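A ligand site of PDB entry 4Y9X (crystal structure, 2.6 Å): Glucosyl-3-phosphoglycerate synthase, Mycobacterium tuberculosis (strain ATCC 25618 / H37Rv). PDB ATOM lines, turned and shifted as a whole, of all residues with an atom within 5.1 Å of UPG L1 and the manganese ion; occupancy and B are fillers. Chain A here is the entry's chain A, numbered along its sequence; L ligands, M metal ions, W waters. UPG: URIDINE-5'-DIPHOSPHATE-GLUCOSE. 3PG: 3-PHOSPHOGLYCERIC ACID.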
ATOM      1  N   PRO A  54     -12.881  26.107  18.282  1.00  0.00           N
ATOM      2  CA  PRO A  54     -13.216  26.991  17.164  1.00  0.00           C
ATOM      3  C   PRO A  54     -13.357  26.167  15.889  1.00  0.00           C
ATOM      4  O   PRO A  54     -12.596  25.223  15.721  1.00  0.00           O
ATOM      5  CB  PRO A  54     -12.014  27.938  17.102  1.00  0.00           C
ATOM      6  CG  PRO A  54     -10.883  27.139  17.653  1.00  0.00           C
ATOM      7  CD  PRO A  54     -11.482  26.250  18.711  1.00  0.00           C
ATOM      8  N   ALA A  55     -14.275  26.532  15.007  1.00  0.00           N
ATOM      9  CA  ALA A  55     -14.487  25.741  13.810  1.00  0.00           C
ATOM     10  C   ALA A  55     -14.939  26.587  12.629  1.00  0.00           C
ATOM     11  O   ALA A  55     -15.912  27.331  12.714  1.00  0.00           O
ATOM     12  CB  ALA A  55     -15.508  24.647  14.082  1.00  0.00           C
ATOM     13  N   LEU A  56     -14.213  26.461  11.523  1.00  0.00           N
ATOM     14  CA  LEU A  56     -14.620  27.044  10.263  1.00  0.00           C
ATOM     15  C   LEU A  56     -14.538  25.959   9.208  1.00  0.00           C
ATOM     16  O   LEU A  56     -13.441  25.603   8.784  1.00  0.00           O
ATOM     17  CB  LEU A  56     -13.720  28.243   9.915  1.00  0.00           C
ATOM     18  CG  LEU A  56     -13.780  28.832   8.506  1.00  0.00           C
ATOM     19  CD1 LEU A  56     -15.168  29.382   8.198  1.00  0.00           C
ATOM     20  CD2 LEU A  56     -12.727  29.924   8.365  1.00  0.00           C
ATOM     21  N   GLU A  58     -15.150  22.568   9.222  1.00  0.00           N
ATOM     22  CA  GLU A  58     -14.439  21.337   9.600  1.00  0.00           C
ATOM     23  C   GLU A  58     -15.330  20.090   9.739  1.00  0.00           C
ATOM     24  O   GLU A  58     -15.178  19.319  10.695  1.00  0.00           O
ATOM     25  CB  GLU A  58     -13.691  21.556  10.906  1.00  0.00           C
ATOM     26  CG  GLU A  58     -12.778  22.771  10.917  1.00  0.00           C
ATOM     27  CD  GLU A  58     -11.602  22.635   9.980  1.00  0.00           C
ATOM     28  OE1 GLU A  58     -11.459  21.583   9.322  1.00  0.00           O
ATOM     29  OE2 GLU A  58     -10.812  23.593   9.896  1.00  0.00           O
ATOM     30  N   LEU A  83     -17.268  26.809  18.791  1.00  0.00           N
ATOM     31  CA  LEU A  83     -17.419  28.174  18.308  1.00  0.00           C
ATOM     32  C   LEU A  83     -17.387  28.179  16.785  1.00  0.00           C
ATOM     33  O   LEU A  83     -16.320  28.115  16.163  1.00  0.00           O
ATOM     34  CB  LEU A  83     -16.324  29.083  18.882  1.00  0.00           C
ATOM     35  CG  LEU A  83     -16.626  30.591  18.912  1.00  0.00           C
ATOM     36  CD1 LEU A  83     -17.228  31.111  17.605  1.00  0.00           C
ATOM     37  CD2 LEU A  83     -17.543  30.935  20.087  1.00  0.00           C
ATOM     38  N   SER A  85     -17.499  29.543  13.199  1.00  0.00           N
ATOM     39  CA  SER A  85     -16.933  30.805  12.737  1.00  0.00           C
ATOM     40  C   SER A  85     -17.442  31.143  11.325  1.00  0.00           C
ATOM     41  O   SER A  85     -16.680  31.626  10.484  1.00  0.00           O
ATOM     42  CB  SER A  85     -15.405  30.721  12.769  1.00  0.00           C
ATOM     43  OG  SER A  85     -14.887  31.235  13.974  1.00  0.00           O
ATOM     44  N   GLY A 117     -11.945  35.872  11.095  1.00  0.00           N
ATOM     45  CA  GLY A 117     -10.664  35.333  11.537  1.00  0.00           C
ATOM     46  C   GLY A 117     -10.741  34.576  12.837  1.00  0.00           C
ATOM     47  O   GLY A 117     -11.705  34.701  13.595  1.00  0.00           O
ATOM     48  N   LYS A 118      -9.698  33.800  13.118  1.00  0.00           N
ATOM     49  CA  LYS A 118      -9.680  32.921  14.285  1.00  0.00           C
ATOM     50  C   LYS A 118      -9.692  33.685  15.603  1.00  0.00           C
ATOM     51  O   LYS A 118     -10.411  33.328  16.540  1.00  0.00           O
ATOM     52  CB  LYS A 118      -8.449  32.002  14.250  1.00  0.00           C
ATOM     53  CG  LYS A 118      -8.591  30.792  15.160  1.00  0.00           C
ATOM     54  CD  LYS A 118      -7.251  30.112  15.404  1.00  0.00           C
ATOM     55  CE  LYS A 118      -7.389  29.037  16.476  1.00  0.00           C
ATOM     56  NZ  LYS A 118      -6.127  28.307  16.739  1.00  0.00           N
ATOM     57  N   ALA A 121     -12.970  34.680  16.955  1.00  0.00           N
ATOM     58  CA  ALA A 121     -13.750  33.559  17.468  1.00  0.00           C
ATOM     59  C   ALA A 121     -13.387  33.222  18.912  1.00  0.00           C
ATOM     60  O   ALA A 121     -14.261  33.032  19.750  1.00  0.00           O
ATOM     61  CB  ALA A 121     -13.565  32.350  16.582  1.00  0.00           C
ATOM     62  N   ASP A 138      -8.023  22.833  18.482  1.00  0.00           N
ATOM     63  CA  ASP A 138      -8.445  23.057  17.109  1.00  0.00           C
ATOM     64  C   ASP A 138      -9.374  21.921  16.682  1.00  0.00           C
ATOM     65  O   ASP A 138      -9.233  20.783  17.141  1.00  0.00           O
ATOM     66  CB  ASP A 138      -7.244  23.143  16.168  1.00  0.00           C
ATOM     67  CG  ASP A 138      -6.494  24.462  16.287  1.00  0.00           C
ATOM     68  OD1 ASP A 138      -6.986  25.380  16.986  1.00  0.00           O
ATOM     69  OD2 ASP A 138      -5.408  24.593  15.673  1.00  0.00           O
ATOM     70  N   SER A 139     -10.320  22.238  15.816  1.00  0.00           N
ATOM     71  CA  SER A 139     -11.350  21.289  15.392  1.00  0.00           C
ATOM     72  C   SER A 139     -10.995  20.532  14.108  1.00  0.00           C
ATOM     73  O   SER A 139     -11.784  19.721  13.627  1.00  0.00           O
ATOM     74  CB  SER A 139     -12.685  22.018  15.231  1.00  0.00           C
ATOM     75  OG  SER A 139     -12.603  23.013  14.231  1.00  0.00           O
ATOM     76  N   ASP A 140      -9.812  20.811  13.546  1.00  0.00           N
ATOM     77  CA  ASP A 140      -9.346  20.112  12.354  1.00  0.00           C
ATOM     78  C   ASP A 140      -8.347  18.982  12.640  1.00  0.00           C
ATOM     79  O   ASP A 140      -7.751  18.437  11.709  1.00  0.00           O
ATOM     80  CB  ASP A 140      -8.725  21.116  11.376  1.00  0.00           C
ATOM     81  CG  ASP A 140      -7.377  21.633  11.820  1.00  0.00           C
ATOM     82  OD1 ASP A 140      -7.126  21.682  13.047  1.00  0.00           O
ATOM     83  OD2 ASP A 140      -6.573  22.003  10.941  1.00  0.00           O
ATOM     84  N   LEU A 213       2.879  28.597  18.195  1.00  0.00           N
ATOM     85  CA  LEU A 213       1.648  28.760  17.413  1.00  0.00           C
ATOM     86  C   LEU A 213       0.619  27.646  17.612  1.00  0.00           C
ATOM     87  O   LEU A 213      -0.392  27.605  16.909  1.00  0.00           O
ATOM     88  CB  LEU A 213       1.985  28.881  15.927  1.00  0.00           C
ATOM     89  CG  LEU A 213       3.034  29.927  15.531  1.00  0.00           C
ATOM     90  CD1 LEU A 213       3.117  30.009  14.018  1.00  0.00           C
ATOM     91  CD2 LEU A 213       2.724  31.300  16.126  1.00  0.00           C
ATOM     92  N   SER A 214       0.877  26.716  18.529  1.00  0.00           N
ATOM     93  CA  SER A 214      -0.012  25.574  18.706  1.00  0.00           C
ATOM     94  C   SER A 214      -1.432  26.008  19.053  1.00  0.00           C
ATOM     95  O   SER A 214      -1.643  26.826  19.943  1.00  0.00           O
ATOM     96  CB  SER A 214       0.531  24.634  19.787  1.00  0.00           C
ATOM     97  OG  SER A 214       0.832  25.345  20.975  1.00  0.00           O
ATOM     98  N   GLY A 215      -2.408  25.454  18.323  1.00  0.00           N
ATOM     99  CA  GLY A 215      -3.808  25.731  18.589  1.00  0.00           C
ATOM    100  C   GLY A 215      -4.384  25.052  19.811  1.00  0.00           C
ATOM    101  O   GLY A 215      -5.532  25.334  20.176  1.00  0.00           O
ATOM    102  N   TYR A 233      -5.081  34.810  12.356  1.00  0.00           N
ATOM    103  CA  TYR A 233      -4.069  33.892  12.875  1.00  0.00           C
ATOM    104  C   TYR A 233      -2.985  34.508  13.782  1.00  0.00           C
ATOM    105  O   TYR A 233      -2.010  33.822  14.115  1.00  0.00           O
ATOM    106  CB  TYR A 233      -3.397  33.199  11.704  1.00  0.00           C
ATOM    107  CG  TYR A 233      -4.341  32.270  10.971  1.00  0.00           C
ATOM    108  CD1 TYR A 233      -4.747  31.084  11.562  1.00  0.00           C
ATOM    109  CD2 TYR A 233      -4.807  32.572   9.710  1.00  0.00           C
ATOM    110  CE1 TYR A 233      -5.605  30.223  10.908  1.00  0.00           C
ATOM    111  CE2 TYR A 233      -5.667  31.727   9.048  1.00  0.00           C
ATOM    112  CZ  TYR A 233      -6.061  30.555   9.652  1.00  0.00           C
ATOM    113  OH  TYR A 233      -6.919  29.695   8.998  1.00  0.00           O
ATOM    114  N   VAL A 235      -3.517  35.499  16.806  1.00  0.00           N
ATOM    115  CA  VAL A 235      -3.989  35.412  18.182  1.00  0.00           C
ATOM    116  C   VAL A 235      -3.049  34.616  19.109  1.00  0.00           C
ATOM    117  O   VAL A 235      -2.816  35.042  20.237  1.00  0.00           O
ATOM    118  CB  VAL A 235      -5.418  34.800  18.246  1.00  0.00           C
ATOM    119  CG1 VAL A 235      -5.494  33.438  17.549  1.00  0.00           C
ATOM    120  CG2 VAL A 235      -5.922  34.711  19.688  1.00  0.00           C
ATOM    121  N   GLU A 236      -2.524  33.485  18.651  1.00  0.00           N
ATOM    122  CA  GLU A 236      -1.648  32.688  19.511  1.00  0.00           C
ATOM    123  C   GLU A 236      -0.340  33.379  19.869  1.00  0.00           C
ATOM    124  O   GLU A 236       0.033  33.422  21.035  1.00  0.00           O
ATOM    125  CB  GLU A 236      -1.293  31.341  18.868  1.00  0.00           C
ATOM    126  CG  GLU A 236      -2.354  30.275  19.027  1.00  0.00           C
ATOM    127  CD  GLU A 236      -3.549  30.484  18.112  1.00  0.00           C
ATOM    128  OE1 GLU A 236      -4.652  30.050  18.495  1.00  0.00           O
ATOM    129  OE2 GLU A 236      -3.390  31.072  17.014  1.00  0.00           O
ATOM    130  N   ILE A 237       0.354  33.908  18.866  1.00  0.00           N
ATOM    131  CA  ILE A 237       1.645  34.536  19.104  1.00  0.00           C
ATOM    132  C   ILE A 237       1.473  35.769  19.982  1.00  0.00           C
ATOM    133  O   ILE A 237       2.309  36.068  20.828  1.00  0.00           O
ATOM    134  CB  ILE A 237       2.348  34.900  17.762  1.00  0.00           C
ATOM    135  CG1 ILE A 237       3.817  35.294  18.016  1.00  0.00           C
ATOM    136  CG2 ILE A 237       1.608  36.001  17.010  1.00  0.00           C
ATOM    137  CD1 ILE A 237       4.698  34.146  18.458  1.00  0.00           C
ATOM    138  N   ARG A 260       0.728  15.138  16.364  1.00  0.00           N
ATOM    139  CA  ARG A 260      -0.512  15.700  15.832  1.00  0.00           C
ATOM    140  C   ARG A 260      -0.509  15.762  14.322  1.00  0.00           C
ATOM    141  O   ARG A 260       0.506  16.024  13.674  1.00  0.00           O
ATOM    142  CB  ARG A 260      -0.801  17.085  16.394  1.00  0.00           C
ATOM    143  CG  ARG A 260       0.169  18.194  15.971  1.00  0.00           C
ATOM    144  CD  ARG A 260      -0.466  19.227  15.038  1.00  0.00           C
ATOM    145  NE  ARG A 260      -1.369  20.141  15.748  1.00  0.00           N
ATOM    146  CZ  ARG A 260      -1.704  21.358  15.318  1.00  0.00           C
ATOM    147  NH1 ARG A 260      -2.524  22.116  16.037  1.00  0.00           N
ATOM    148  NH2 ARG A 260      -1.228  21.821  14.166  1.00  0.00           N
ATOM    149  N   HIS A 262      -3.119  17.259  11.060  1.00  0.00           N
ATOM    150  CA  HIS A 262      -4.219  18.166  10.740  1.00  0.00           C
ATOM    151  C   HIS A 262      -4.221  18.466   9.252  1.00  0.00           C
ATOM    152  O   HIS A 262      -3.394  17.962   8.493  1.00  0.00           O
ATOM    153  CB  HIS A 262      -4.124  19.464  11.563  1.00  0.00           C
ATOM    154  CG  HIS A 262      -2.970  20.350  11.202  1.00  0.00           C
ATOM    155  ND1 HIS A 262      -3.121  21.696  10.922  1.00  0.00           N
ATOM    156  CD2 HIS A 262      -1.644  20.095  11.083  1.00  0.00           C
ATOM    157  CE1 HIS A 262      -1.944  22.223  10.643  1.00  0.00           C
ATOM    158  NE2 HIS A 262      -1.026  21.270  10.733  1.00  0.00           N
ATOM    159  N   ARG A 263      -5.192  19.267   8.840  1.00  0.00           N
ATOM    160  CA  ARG A 263      -5.271  19.780   7.478  1.00  0.00           C
ATOM    161  C   ARG A 263      -3.954  20.402   7.063  1.00  0.00           C
ATOM    162  O   ARG A 263      -3.461  21.306   7.749  1.00  0.00           O
ATOM    163  CB  ARG A 263      -6.381  20.830   7.402  1.00  0.00           C
ATOM    164  CG  ARG A 263      -6.836  21.189   5.994  1.00  0.00           C
ATOM    165  CD  ARG A 263      -7.391  22.611   5.907  1.00  0.00           C
ATOM    166  NE  ARG A 263      -8.217  22.980   7.063  1.00  0.00           N
ATOM    167  CZ  ARG A 263      -7.810  23.694   8.108  1.00  0.00           C
ATOM    168  NH1 ARG A 263      -6.561  24.149   8.183  1.00  0.00           N
ATOM    169  NH2 ARG A 263      -8.648  23.955   9.095  1.00  0.00           N
ATOM    170  N   ARG A 265      -2.727  22.925   4.628  1.00  0.00           N
ATOM    171  CA  ARG A 265      -3.121  24.021   3.771  1.00  0.00           C
ATOM    172  C   ARG A 265      -2.129  24.280   2.624  1.00  0.00           C
ATOM    173  O   ARG A 265      -0.944  23.977   2.757  1.00  0.00           O
ATOM    174  CB  ARG A 265      -3.314  25.268   4.629  1.00  0.00           C
ATOM    175  CG  ARG A 265      -4.333  25.011   5.735  1.00  0.00           C
ATOM    176  CD  ARG A 265      -4.507  26.210   6.612  1.00  0.00           C
ATOM    177  NE  ARG A 265      -5.212  27.282   5.909  1.00  0.00           N
ATOM    178  CZ  ARG A 265      -5.123  28.569   6.217  1.00  0.00           C
ATOM    179  NH1 ARG A 265      -4.346  28.962   7.220  1.00  0.00           N
ATOM    180  NH2 ARG A 265      -5.797  29.472   5.522  1.00  0.00           N
ATOM    181  N   LEU A 270      -0.758  29.789   3.665  1.00  0.00           N
ATOM    182  CA  LEU A 270       0.259  29.941   4.697  1.00  0.00           C
ATOM    183  C   LEU A 270       0.928  31.308   4.609  1.00  0.00           C
ATOM    184  O   LEU A 270       1.400  31.841   5.605  1.00  0.00           O
ATOM    185  CB  LEU A 270       1.293  28.829   4.604  1.00  0.00           C
ATOM    186  CG  LEU A 270       0.786  27.402   4.847  1.00  0.00           C
ATOM    187  CD1 LEU A 270       1.952  26.432   4.876  1.00  0.00           C
ATOM    188  CD2 LEU A 270      -0.039  27.304   6.132  1.00  0.00           C
ATOM    189  N   MET A 273      -1.136  33.688   6.434  1.00  0.00           N
ATOM    190  CA  MET A 273      -1.122  33.404   7.862  1.00  0.00           C
ATOM    191  C   MET A 273       0.147  33.989   8.479  1.00  0.00           C
ATOM    192  O   MET A 273       0.099  34.659   9.517  1.00  0.00           O
ATOM    193  CB  MET A 273      -1.156  31.903   8.117  1.00  0.00           C
ATOM    194  CG  MET A 273      -1.418  31.510   9.553  1.00  0.00           C
ATOM    195  SD  MET A 273      -0.699  29.921   9.993  1.00  0.00           S
ATOM    196  CE  MET A 273      -1.538  28.880   8.817  1.00  0.00           C
ATOM    197  N   VAL A 277       0.941  36.830  11.410  1.00  0.00           N
ATOM    198  CA  VAL A 277       1.743  36.454  12.573  1.00  0.00           C
ATOM    199  C   VAL A 277       2.861  37.479  12.733  1.00  0.00           C
ATOM    200  O   VAL A 277       3.153  37.930  13.834  1.00  0.00           O
ATOM    201  CB  VAL A 277       2.335  35.032  12.412  1.00  0.00           C
ATOM    202  CG1 VAL A 277       3.488  34.776  13.395  1.00  0.00           C
ATOM    203  CG2 VAL A 277       1.245  33.983  12.570  1.00  0.00           C
HETATM  204  N1  UPG L   1     -10.488  28.700  12.542  1.00  0.00           N
HETATM  205  C2  UPG L   1     -11.641  29.480  12.811  1.00  0.00           C
HETATM  206  N3  UPG L   1     -11.860  30.612  12.114  1.00  0.00           N
HETATM  207  C4  UPG L   1     -11.015  31.029  11.166  1.00  0.00           C
HETATM  208  C5  UPG L   1      -9.871  30.277  10.890  1.00  0.00           C
HETATM  209  C6  UPG L   1      -9.626  29.110  11.602  1.00  0.00           C
HETATM  210  O2  UPG L   1     -12.458  29.135  13.691  1.00  0.00           O
HETATM  211  O4  UPG L   1     -11.242  32.075  10.534  1.00  0.00           O
HETATM  212  C1C UPG L   1     -10.234  27.465  13.297  1.00  0.00           C
HETATM  213  C2C UPG L   1     -10.234  26.236  12.410  1.00  0.00           C
HETATM  214  O2C UPG L   1     -11.525  25.637  12.394  1.00  0.00           O
HETATM  215  C3C UPG L   1      -9.204  25.318  13.041  1.00  0.00           C
HETATM  216  C4C UPG L   1      -8.357  26.217  13.924  1.00  0.00           C
HETATM  217  O4C UPG L   1      -8.948  27.521  13.907  1.00  0.00           O
HETATM  218  O3C UPG L   1      -9.841  24.301  13.818  1.00  0.00           O
HETATM  219  C5C UPG L   1      -6.934  26.318  13.400  1.00  0.00           C
HETATM  220  O5C UPG L   1      -6.951  26.968  12.127  1.00  0.00           O
HETATM  221  PA  UPG L   1      -6.121  26.386  10.873  1.00  0.00           P
HETATM  222  O1A UPG L   1      -6.064  24.881  10.912  1.00  0.00           O
HETATM  223  O2A UPG L   1      -6.733  26.875   9.586  1.00  0.00           O
HETATM  224  O3A UPG L   1      -4.675  27.057  11.100  1.00  0.00           O
HETATM  225  PB  UPG L   1      -3.309  26.228  11.035  1.00  0.00           P
HETATM  226  O1B UPG L   1      -2.790  26.157   9.618  1.00  0.00           O
HETATM  227  O2B UPG L   1      -3.467  24.839  11.622  1.00  0.00           O
HETATM  228  O3B UPG L   1      -2.414  27.184  11.968  1.00  0.00           O
HETATM  229  C1' UPG L   1      -1.646  26.774  13.098  1.00  0.00           C
HETATM  230  C2' UPG L   1      -2.522  26.336  14.266  1.00  0.00           C
HETATM  231  C3' UPG L   1      -3.537  27.430  14.574  1.00  0.00           C
HETATM  232  C4' UPG L   1      -2.827  28.748  14.829  1.00  0.00           C
HETATM  233  C5' UPG L   1      -1.798  29.059  13.724  1.00  0.00           C
HETATM  234  C6' UPG L   1      -0.986  30.319  14.010  1.00  0.00           C
HETATM  235  O2' UPG L   1      -3.185  25.092  13.956  1.00  0.00           O
HETATM  236  O3' UPG L   1      -4.274  27.075  15.749  1.00  0.00           O
HETATM  237  O4' UPG L   1      -3.797  29.815  14.871  1.00  0.00           O
HETATM  238  O5' UPG L   1      -0.926  27.934  13.512  1.00  0.00           O
HETATM  239  O6' UPG L   1      -0.944  30.605  15.412  1.00  0.00           O
HETATM  240  C1  3PG L   2       1.939  25.811  11.556  1.00  0.00           C
HETATM  241  O1  3PG L   2       1.393  25.457  12.629  1.00  0.00           O
HETATM  242  O2  3PG L   2       3.059  26.374  11.576  1.00  0.00           O
HETATM  243  C2  3PG L   2       1.250  25.568  10.229  1.00  0.00           C
HETATM  244  O3  3PG L   2       0.043  24.857  10.435  1.00  0.00           O
HETATM  245  C3  3PG L   2       2.163  24.751   9.338  1.00  0.00           C
HETATM  246  O1P 3PG L   2       1.472  23.624   8.867  1.00  0.00           O
HETATM  247  P   3PG L   2       2.317  22.335   8.493  1.00  0.00           P
HETATM  248  O2P 3PG L   2       1.434  21.325   7.808  1.00  0.00           O
HETATM  249  O3P 3PG L   2       3.459  22.735   7.578  1.00  0.00           O
HETATM  250  O4P 3PG L   2       2.879  21.731   9.757  1.00  0.00           O
HETATM  251 MN    MN M   1      -4.773  23.119  11.342  1.00  0.00          MN
HETATM  252  O   HOH W   1      -5.071  22.894  13.521  1.00  0.00           O
HETATM  253  O   HOH W   2      -4.612  23.511   9.198  1.00  0.00           O
HETATM  254  O   HOH W   3      -0.618  33.598  16.459  1.00  0.00           O
HETATM  255  O   HOH W   4     -13.929  33.851   9.486  1.00  0.00           O
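OE2 of Glu 58 lies within hydrogen-bond range of O2C of UPG L1, at 3.3 Å.
An oxygen (O3') of UPG L1 lies within hydrogen-bond range of the side-chain amino group (NZ) of Lys 118 (2.4 Å).
O2 of UPG L1 lies within hydrogen-bond range of N of Ala 55 (3.4 Å).
N of Lys 118 lies within hydrogen-bond range of O4 of UPG L1.
OE2 of Glu 236 is in hydrogen-bond range of O4' of UPG L1, 2.5 Å away.
The guanidinium group (NH1) of Arg 265 is in salt-bridge range of an oxygen (O2A) of UPG L1.
An oxygen (O6') of UPG L1 is in hydrogen-bond range of the backbone carbonyl oxygen (O) of Leu 213 (3.4 Å).
The side-chain hydroxyl of Ser 85 sits at hydrogen-bond distance from an oxygen (O2) of UPG L1 (3.2 Å).
NH1 of Arg 263 lies within salt-bridge range of O2A of UPG L1.
An oxygen (O2C) of UPG L1 sits at hydrogen-bond distance from the backbone NH (N) of Leu 56, at 2.9 Å.
The side-chain hydroxyl (OG) of Ser 139 lies within hydrogen-bond range of an oxygen (O3C) of UPG L1 (3.1 Å).
N of Ser 139 sits at hydrogen-bond distance from O3C of UPG L1, 2.9 Å away.
OH of Tyr 233 is in hydrogen-bond range of O2A of UPG L1 (2.9 Å).
An oxygen (O3C) of UPG L1 is in hydrogen-bond range of the backbone carbonyl oxygen (O) of Pro 54 (3.5 Å).
An oxygen (O3') of UPG L1 sits at hydrogen-bond distance from the side-chain carboxylate of Asp 138 (2.7 Å).
An oxygen (O1B) of UPG L1 lies within hydrogen-bond range of an oxygen (O3) of 3PG L2.
The side-chain carboxylate (OE1) of Glu 58 is in salt-bridge range of the guanidinium group (NH2) of Arg 263 (3.7 Å).
NE2 of His 262 sits at hydrogen-bond distance from NH2 of Arg 260.
The side-chain amino group (NZ) of Lys 118 is in salt-bridge range of the side-chain carboxylate (OE1) of Glu 236 (2.9 Å).
The backbone carbonyl oxygen (O) of Pro 54 lies within hydrogen-bond range of the side-chain hydroxyl (OG) of Ser 139.
N of Ala 55 sits at hydrogen-bond distance from O of Leu 83 (2.8 Å).
The side-chain carboxylate (OD2) of Asp 138 lies within salt-bridge range of the guanidinium group (NH1) of Arg 260 (3.8 Å).
The side-chain carboxylate of Asp 138 is in salt-bridge range of the side-chain amino group of Lys 118, at 3.1 Å.
The side-chain carboxylate (OD2) of Asp 140 lies close to the guanidinium group (NH2) of Arg 263 (3.4 Å).
An oxygen (O3B) of UPG L1 lies close to the side-chain sulfur (SD) of Met 273 (3.8 Å).
Merely in contact with UPG L1: Gly 215 (3.2 Å), Gly 117 (3.4 Å) and Arg 260 (3.7 Å).
Hydrophobic or aromatic side chains that line UPG L1: Pro 54, Leu 56, Leu 213, Tyr 233, His 262 and Met 273.
19 residues have an atom within 4 Å of UPG L1: Pro 54, Ala 55, Leu 56, Glu 58, Ser 85, Gly 117, Lys 118, Asp 138, Ser 139, Asp 140, Leu 213, Gly 215, Tyr 233, Glu 236, Arg 260, His 262, Arg 263, Arg 265 and Met 273.
The nearest printed residue that does not touch UPG L1 is Ala 121 (4.5 Å).
NH1 of Arg 263 touches the manganese ion, 3.8 Å away.
Of the 26 residues printed, 3 come within 4 Å of the manganese ion.
The manganese ion is bound by OD2 of Asp 140 (2.2 Å), O2B of UPG L1 (2.2 Å), water W2 (2.2 Å), water W1 (2.2 Å), ND1 of His 262 (2.2 Å) and O1A of UPG L1 (2.2 Å).
The manganese ion has six donor atoms within binding distance.
Water W2 bridges O of Arg 263 (2.9 Å) and O1B of UPG L1 (3.2 Å).
Water W1 lies within hydrogen-bond range of the side-chain carboxylate of Asp 140 (2.4 Å), the side-chain carboxylate of Asp 138 (2.8 Å) and an oxygen (O2') of UPG L1 (2.9 Å).
Water W4 bridges the backbone NH (N) of Gly 117 and an oxygen (O4) of UPG L1.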
